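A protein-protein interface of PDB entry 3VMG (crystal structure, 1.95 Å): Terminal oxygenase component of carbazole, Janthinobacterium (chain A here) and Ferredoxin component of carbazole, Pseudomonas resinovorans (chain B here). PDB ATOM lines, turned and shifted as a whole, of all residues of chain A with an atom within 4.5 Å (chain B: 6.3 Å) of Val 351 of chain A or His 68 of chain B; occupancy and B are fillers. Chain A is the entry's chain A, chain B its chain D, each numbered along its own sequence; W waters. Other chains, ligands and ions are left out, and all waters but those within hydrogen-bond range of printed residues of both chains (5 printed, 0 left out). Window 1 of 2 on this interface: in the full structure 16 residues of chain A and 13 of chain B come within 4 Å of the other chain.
The side-chain carboxylate of Glu 353 of chain A sits at hydrogen-bond distance from a ring nitrogen (NE2) of His 68 of chain B (2.9 Å).
O of Arg 11 of chain A sits close to O of Phe 67 of chain B, at 3.5 Å.
NH1 of Arg 11 of chain A is in hydrogen-bond range of O of His 68 of chain B.
O of Asn 352 of chain A lies within hydrogen-bond range of NE2 of His 48 of chain B (3.3 Å).
O of Ser 82 of chain B is in hydrogen-bond range of NH1 of Arg 11 of chain A (2.9 Å).
The backbone carbonyl oxygen of Glu 353 of chain A lies close to a ring nitrogen (NE2) of His 48 of chain B (3.3 Å).
The backbone carbonyl oxygen of Gly 69 of chain B lies close to the guanidinium group of Arg 11 of chain A.
N of Phe 67 of chain B lies close to SG of Cys 65 of chain B, at 3.5 Å.
The side-chain amide nitrogen (ND2) of Asn 352 of chain A is in hydrogen-bond range of the backbone carbonyl oxygen (O) of Lys 348 of chain A (3.3 Å).
N of Cys 65 of chain B is in hydrogen-bond range of O of Gly 70 of chain B, 2.7 Å away.
Among the printed residues, merely in contact across the chains: Arg 11 of chain A with Pro 66 of chain B, Arg 11 of chain A with Gly 70 of chain B, Arg 11 of chain A with Pro 83 of chain B, Trp 15 of chain A with Phe 67 of chain B, Trp 350 of chain A with His 68 of chain B, Val 351 of chain A with His 48 of chain B, Val 351 of chain A with His 68 of chain B, Val 351 of chain A with Pro 83 of chain B and Asn 352 of chain A with Pro 83 of chain B.
Val 351 of chain A touches just these residues of chain B: His 48, His 68 and Pro 83.
Of chain A, only Arg 11, Trp 350, Val 351 and Glu 353 come within 4 Å of His 68 of chain B.
Of the printed residues of chain A, Pro 66 of chain B touches Arg 11.
Printed residues of chain B within 4 Å of Asn 352 of chain A: His 48 and Pro 83.
Gly 49 of chain B touches none of the printed residues of chain A.
The nearest residue of chain B that does not touch Val 351 of chain A is Ser 82 of chain B (5.7 Å).
Hydrophobic or aromatic side chains of chain A that line the printed part of chain B: Trp 15 and Val 351.
Printed residues of chain B that touch a printed residue of chain A: His 48, Pro 66, Phe 67, His 68, Gly 69, Gly 70, Ser 82 and Pro 83.
Hydrophobic or aromatic side chains of chain B within 4 Å of the printed part of chain A: His 48, Phe 67, His 68 and Pro 83.
Among the printed residues, no Asp or Glu carboxylate lies within 4 Å of a Lys or Arg side-chain nitrogen of the other chain.
Water W1 bridges the backbone carbonyl oxygen (O) of Glu 353 of chain A (2.6 Å) and the backbone carbonyl oxygen (O) of His 48 of chain B (2.7 Å).
Water W5 lies within hydrogen-bond range of OG of Ser 82 of chain B (2.7 Å) and NH2 of Arg 11 of chain A (3.1 Å).
Water W3 lies within hydrogen-bond range of O of Phe 67 of chain B (2.7 Å) and N of Trp 15 of chain A (3.5 Å).
Water W2 lies within hydrogen-bond range of O of Arg 11 of chain A (2.8 Å), O of Cys 65 of chain B (2.8 Å) and N of Gly 69 of chain B (3.4 Å).
Water W4 lies within hydrogen-bond range of O of Asn 352 of chain A and NE2 of His 48 of chain B.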
ATOM      1  N   ILE A   8     -28.384 -18.230   6.664  1.00  0.00           N
ATOM      2  CA  ILE A   8     -28.266 -18.316   5.213  1.00  0.00           C
ATOM      3  C   ILE A   8     -27.128 -17.418   4.740  1.00  0.00           C
ATOM      4  O   ILE A   8     -26.292 -17.833   3.939  1.00  0.00           O
ATOM      5  CB  ILE A   8     -29.578 -17.891   4.514  1.00  0.00           C
ATOM      6  CG1 ILE A   8     -30.691 -18.886   4.862  1.00  0.00           C
ATOM      7  CG2 ILE A   8     -29.363 -17.803   3.007  1.00  0.00           C
ATOM      8  CD1 ILE A   8     -32.042 -18.547   4.254  1.00  0.00           C
ATOM      9  N   ARG A  11     -23.693 -18.767   5.035  1.00  0.00           N
ATOM     10  CA  ARG A  11     -23.389 -19.792   4.045  1.00  0.00           C
ATOM     11  C   ARG A  11     -22.912 -19.250   2.698  1.00  0.00           C
ATOM     12  O   ARG A  11     -22.018 -19.826   2.078  1.00  0.00           O
ATOM     13  CB  ARG A  11     -24.617 -20.678   3.815  1.00  0.00           C
ATOM     14  CG  ARG A  11     -24.721 -21.878   4.747  1.00  0.00           C
ATOM     15  CD  ARG A  11     -26.065 -22.569   4.577  1.00  0.00           C
ATOM     16  NE  ARG A  11     -26.131 -23.856   5.265  1.00  0.00           N
ATOM     17  CZ  ARG A  11     -25.574 -24.977   4.815  1.00  0.00           C
ATOM     18  NH1 ARG A  11     -24.901 -24.983   3.670  1.00  0.00           N
ATOM     19  NH2 ARG A  11     -25.696 -26.097   5.514  1.00  0.00           N
ATOM     20  N   TRP A  15     -21.131 -13.934  -1.861  1.00  0.00           N
ATOM     21  CA  TRP A  15     -21.957 -12.767  -2.155  1.00  0.00           C
ATOM     22  C   TRP A  15     -23.111 -12.528  -1.176  1.00  0.00           C
ATOM     23  O   TRP A  15     -24.257 -12.315  -1.593  1.00  0.00           O
ATOM     24  CB  TRP A  15     -22.499 -12.944  -3.582  1.00  0.00           C
ATOM     25  CG  TRP A  15     -23.126 -14.302  -3.835  1.00  0.00           C
ATOM     26  CD1 TRP A  15     -24.369 -14.714  -3.450  1.00  0.00           C
ATOM     27  CD2 TRP A  15     -22.523 -15.422  -4.498  1.00  0.00           C
ATOM     28  NE1 TRP A  15     -24.580 -16.017  -3.831  1.00  0.00           N
ATOM     29  CE2 TRP A  15     -23.461 -16.476  -4.475  1.00  0.00           C
ATOM     30  CE3 TRP A  15     -21.277 -15.636  -5.110  1.00  0.00           C
ATOM     31  CZ2 TRP A  15     -23.196 -17.732  -5.038  1.00  0.00           C
ATOM     32  CZ3 TRP A  15     -21.014 -16.885  -5.670  1.00  0.00           C
ATOM     33  CH2 TRP A  15     -21.968 -17.916  -5.630  1.00  0.00           C
ATOM     34  N   ASP A 347     -35.835 -17.824   0.549  1.00  0.00           N
ATOM     35  CA  ASP A 347     -34.395 -17.556   0.592  1.00  0.00           C
ATOM     36  C   ASP A 347     -33.549 -18.835   0.532  1.00  0.00           C
ATOM     37  O   ASP A 347     -32.317 -18.768   0.560  1.00  0.00           O
ATOM     38  CB  ASP A 347     -34.012 -16.749   1.847  1.00  0.00           C
ATOM     39  CG  ASP A 347     -34.550 -15.320   1.823  1.00  0.00           C
ATOM     40  OD1 ASP A 347     -34.467 -14.657   0.762  1.00  0.00           O
ATOM     41  OD2 ASP A 347     -35.041 -14.846   2.871  1.00  0.00           O
ATOM     42  N   LYS A 348     -34.203 -19.992   0.433  1.00  0.00           N
ATOM     43  CA  LYS A 348     -33.491 -21.274   0.385  1.00  0.00           C
ATOM     44  C   LYS A 348     -32.823 -21.569  -0.964  1.00  0.00           C
ATOM     45  O   LYS A 348     -31.812 -22.276  -1.027  1.00  0.00           O
ATOM     46  CB  LYS A 348     -34.446 -22.411   0.767  1.00  0.00           C
ATOM     47  CG  LYS A 348     -34.397 -22.826   2.241  1.00  0.00           C
ATOM     48  CD  LYS A 348     -34.270 -21.645   3.184  1.00  0.00           C
ATOM     49  CE  LYS A 348     -33.991 -22.093   4.626  1.00  0.00           C
ATOM     50  NZ  LYS A 348     -35.082 -22.915   5.234  1.00  0.00           N
ATOM     51  N   GLY A 349     -33.386 -21.030  -2.041  1.00  0.00           N
ATOM     52  CA  GLY A 349     -32.803 -21.247  -3.353  1.00  0.00           C
ATOM     53  C   GLY A 349     -31.388 -20.687  -3.454  1.00  0.00           C
ATOM     54  O   GLY A 349     -30.584 -21.174  -4.253  1.00  0.00           O
ATOM     55  N   TRP A 350     -31.075 -19.671  -2.651  1.00  0.00           N
ATOM     56  CA  TRP A 350     -29.740 -19.063  -2.667  1.00  0.00           C
ATOM     57  C   TRP A 350     -28.704 -20.035  -2.098  1.00  0.00           C
ATOM     58  O   TRP A 350     -27.499 -19.795  -2.162  1.00  0.00           O
ATOM     59  CB  TRP A 350     -29.723 -17.755  -1.858  1.00  0.00           C
ATOM     60  CG  TRP A 350     -30.635 -16.690  -2.401  1.00  0.00           C
ATOM     61  CD1 TRP A 350     -31.779 -16.217  -1.818  1.00  0.00           C
ATOM     62  CD2 TRP A 350     -30.493 -15.982  -3.637  1.00  0.00           C
ATOM     63  NE1 TRP A 350     -32.355 -15.258  -2.614  1.00  0.00           N
ATOM     64  CE2 TRP A 350     -31.588 -15.094  -3.738  1.00  0.00           C
ATOM     65  CE3 TRP A 350     -29.545 -16.012  -4.674  1.00  0.00           C
ATOM     66  CZ2 TRP A 350     -31.765 -14.239  -4.834  1.00  0.00           C
ATOM     67  CZ3 TRP A 350     -29.720 -15.165  -5.766  1.00  0.00           C
ATOM     68  CH2 TRP A 350     -30.825 -14.287  -5.835  1.00  0.00           C
ATOM     69  N   VAL A 351     -29.191 -21.131  -1.526  1.00  0.00           N
ATOM     70  CA  VAL A 351     -28.319 -22.160  -0.973  1.00  0.00           C
ATOM     71  C   VAL A 351     -28.398 -23.447  -1.792  1.00  0.00           C
ATOM     72  O   VAL A 351     -27.381 -24.091  -2.062  1.00  0.00           O
ATOM     73  CB  VAL A 351     -28.714 -22.520   0.479  1.00  0.00           C
ATOM     74  CG1 VAL A 351     -27.874 -23.700   0.967  1.00  0.00           C
ATOM     75  CG2 VAL A 351     -28.528 -21.316   1.390  1.00  0.00           C
ATOM     76  N   ASN A 352     -29.609 -23.808  -2.207  1.00  0.00           N
ATOM     77  CA  ASN A 352     -29.824 -25.061  -2.929  1.00  0.00           C
ATOM     78  C   ASN A 352     -29.636 -25.126  -4.445  1.00  0.00           C
ATOM     79  O   ASN A 352     -29.541 -26.221  -5.004  1.00  0.00           O
ATOM     80  CB  ASN A 352     -31.197 -25.611  -2.545  1.00  0.00           C
ATOM     81  CG  ASN A 352     -31.288 -25.917  -1.065  1.00  0.00           C
ATOM     82  OD1 ASN A 352     -30.404 -26.571  -0.515  1.00  0.00           O
ATOM     83  ND2 ASN A 352     -32.345 -25.443  -0.410  1.00  0.00           N
ATOM     84  N   GLU A 353     -29.586 -23.971  -5.100  1.00  0.00           N
ATOM     85  CA  GLU A 353     -29.383 -23.898  -6.547  1.00  0.00           C
ATOM     86  C   GLU A 353     -28.143 -24.704  -6.956  1.00  0.00           C
ATOM     87  O   GLU A 353     -27.113 -24.643  -6.288  1.00  0.00           O
ATOM     88  CB  GLU A 353     -29.165 -22.437  -6.966  1.00  0.00           C
ATOM     89  CG  GLU A 353     -28.012 -21.776  -6.190  1.00  0.00           C
ATOM     90  CD  GLU A 353     -27.771 -20.308  -6.517  1.00  0.00           C
ATOM     91  OE1 GLU A 353     -28.676 -19.632  -7.059  1.00  0.00           O
ATOM     92  OE2 GLU A 353     -26.661 -19.821  -6.199  1.00  0.00           O
ATOM     93  N   HIS B  48     -21.477 -29.671  -5.953  1.00  0.00           N
ATOM     94  CA  HIS B  48     -22.788 -29.025  -5.911  1.00  0.00           C
ATOM     95  C   HIS B  48     -22.924 -27.870  -6.906  1.00  0.00           C
ATOM     96  O   HIS B  48     -24.013 -27.325  -7.088  1.00  0.00           O
ATOM     97  CB  HIS B  48     -23.067 -28.523  -4.487  1.00  0.00           C
ATOM     98  CG  HIS B  48     -24.364 -27.784  -4.338  1.00  0.00           C
ATOM     99  ND1 HIS B  48     -24.429 -26.412  -4.194  1.00  0.00           N
ATOM    100  CD2 HIS B  48     -25.645 -28.225  -4.312  1.00  0.00           C
ATOM    101  CE1 HIS B  48     -25.694 -26.043  -4.083  1.00  0.00           C
ATOM    102  NE2 HIS B  48     -26.451 -27.123  -4.152  1.00  0.00           N
ATOM    103  N   GLY B  49     -21.824 -27.494  -7.550  1.00  0.00           N
ATOM    104  CA  GLY B  49     -21.883 -26.396  -8.498  1.00  0.00           C
ATOM    105  C   GLY B  49     -20.578 -26.114  -9.213  1.00  0.00           C
ATOM    106  O   GLY B  49     -19.967 -27.019  -9.773  1.00  0.00           O
ATOM    107  N   ALA B  51     -18.078 -23.915  -7.649  1.00  0.00           N
ATOM    108  CA  ALA B  51     -17.157 -23.286  -6.705  1.00  0.00           C
ATOM    109  C   ALA B  51     -15.803 -23.993  -6.631  1.00  0.00           C
ATOM    110  O   ALA B  51     -15.692 -25.182  -6.924  1.00  0.00           O
ATOM    111  CB  ALA B  51     -17.784 -23.253  -5.319  1.00  0.00           C
ATOM    112  N   CYS B  65     -17.318 -25.438   1.394  1.00  0.00           N
ATOM    113  CA  CYS B  65     -17.375 -24.698   0.137  1.00  0.00           C
ATOM    114  C   CYS B  65     -17.773 -23.238   0.381  1.00  0.00           C
ATOM    115  O   CYS B  65     -18.693 -22.958   1.143  1.00  0.00           O
ATOM    116  CB  CYS B  65     -18.379 -25.365  -0.805  1.00  0.00           C
ATOM    117  SG  CYS B  65     -18.644 -24.469  -2.334  1.00  0.00           S
ATOM    118  N   PRO B  66     -17.085 -22.290  -0.281  1.00  0.00           N
ATOM    119  CA  PRO B  66     -17.339 -20.850  -0.150  1.00  0.00           C
ATOM    120  C   PRO B  66     -18.631 -20.329  -0.784  1.00  0.00           C
ATOM    121  O   PRO B  66     -19.083 -19.227  -0.463  1.00  0.00           O
ATOM    122  CB  PRO B  66     -16.104 -20.235  -0.795  1.00  0.00           C
ATOM    123  CG  PRO B  66     -15.827 -21.187  -1.906  1.00  0.00           C
ATOM    124  CD  PRO B  66     -15.974 -22.533  -1.218  1.00  0.00           C
ATOM    125  N   PHE B  67     -19.230 -21.110  -1.676  1.00  0.00           N
ATOM    126  CA  PHE B  67     -20.447 -20.658  -2.339  1.00  0.00           C
ATOM    127  C   PHE B  67     -21.748 -20.872  -1.567  1.00  0.00           C
ATOM    128  O   PHE B  67     -22.489 -19.917  -1.341  1.00  0.00           O
ATOM    129  CB  PHE B  67     -20.545 -21.284  -3.737  1.00  0.00           C
ATOM    130  CG  PHE B  67     -19.729 -20.564  -4.786  1.00  0.00           C
ATOM    131  CD1 PHE B  67     -18.657 -19.752  -4.426  1.00  0.00           C
ATOM    132  CD2 PHE B  67     -20.021 -20.718  -6.141  1.00  0.00           C
ATOM    133  CE1 PHE B  67     -17.884 -19.104  -5.399  1.00  0.00           C
ATOM    134  CE2 PHE B  67     -19.256 -20.078  -7.120  1.00  0.00           C
ATOM    135  CZ  PHE B  67     -18.189 -19.272  -6.753  1.00  0.00           C
ATOM    136  N   HIS B  68     -22.036 -22.104  -1.156  1.00  0.00           N
ATOM    137  CA  HIS B  68     -23.280 -22.351  -0.432  1.00  0.00           C
ATOM    138  C   HIS B  68     -23.114 -22.978   0.948  1.00  0.00           C
ATOM    139  O   HIS B  68     -24.097 -23.271   1.623  1.00  0.00           O
ATOM    140  CB  HIS B  68     -24.221 -23.206  -1.282  1.00  0.00           C
ATOM    141  CG  HIS B  68     -24.473 -22.644  -2.649  1.00  0.00           C
ATOM    142  ND1 HIS B  68     -23.983 -23.230  -3.796  1.00  0.00           N
ATOM    143  CD2 HIS B  68     -25.146 -21.538  -3.051  1.00  0.00           C
ATOM    144  CE1 HIS B  68     -24.342 -22.511  -4.846  1.00  0.00           C
ATOM    145  NE2 HIS B  68     -25.050 -21.478  -4.422  1.00  0.00           N
ATOM    146  N   GLY B  69     -21.873 -23.182   1.372  1.00  0.00           N
ATOM    147  CA  GLY B  69     -21.649 -23.748   2.694  1.00  0.00           C
ATOM    148  C   GLY B  69     -21.686 -25.263   2.789  1.00  0.00           C
ATOM    149  O   GLY B  69     -21.661 -25.815   3.894  1.00  0.00           O
ATOM    150  N   GLY B  70     -21.774 -25.940   1.647  1.00  0.00           N
ATOM    151  CA  GLY B  70     -21.763 -27.395   1.663  1.00  0.00           C
ATOM    152  C   GLY B  70     -20.374 -27.818   2.126  1.00  0.00           C
ATOM    153  O   GLY B  70     -19.455 -27.002   2.116  1.00  0.00           O
ATOM    154  N   SER B  82     -24.980 -30.198   4.098  1.00  0.00           N
ATOM    155  CA  SER B  82     -25.885 -29.906   2.991  1.00  0.00           C
ATOM    156  C   SER B  82     -25.384 -28.568   2.436  1.00  0.00           C
ATOM    157  O   SER B  82     -24.680 -27.834   3.134  1.00  0.00           O
ATOM    158  CB  SER B  82     -27.317 -29.762   3.509  1.00  0.00           C
ATOM    159  OG  SER B  82     -27.368 -28.855   4.596  1.00  0.00           O
ATOM    160  N   PRO B  83     -25.745 -28.220   1.188  1.00  0.00           N
ATOM    161  CA  PRO B  83     -26.588 -28.940   0.227  1.00  0.00           C
ATOM    162  C   PRO B  83     -25.873 -30.038  -0.568  1.00  0.00           C
ATOM    163  O   PRO B  83     -26.500 -30.723  -1.373  1.00  0.00           O
ATOM    164  CB  PRO B  83     -27.088 -27.820  -0.681  1.00  0.00           C
ATOM    165  CG  PRO B  83     -25.872 -26.944  -0.780  1.00  0.00           C
ATOM    166  CD  PRO B  83     -25.408 -26.877   0.677  1.00  0.00           C
HETATM  167  O   HOH W   1     -24.625 -24.682  -7.190  1.00  0.00           O
HETATM  168  O   HOH W   2     -19.677 -21.034   2.922  1.00  0.00           O
HETATM  169  O   HOH W   3     -21.694 -17.377  -2.016  1.00  0.00           O
HETATM  170  O   HOH W   4     -29.040 -28.709  -3.653  1.00  0.00           O
HETATM  171  O   HOH W   5     -28.091 -26.512   3.543  1.00  0.00           O
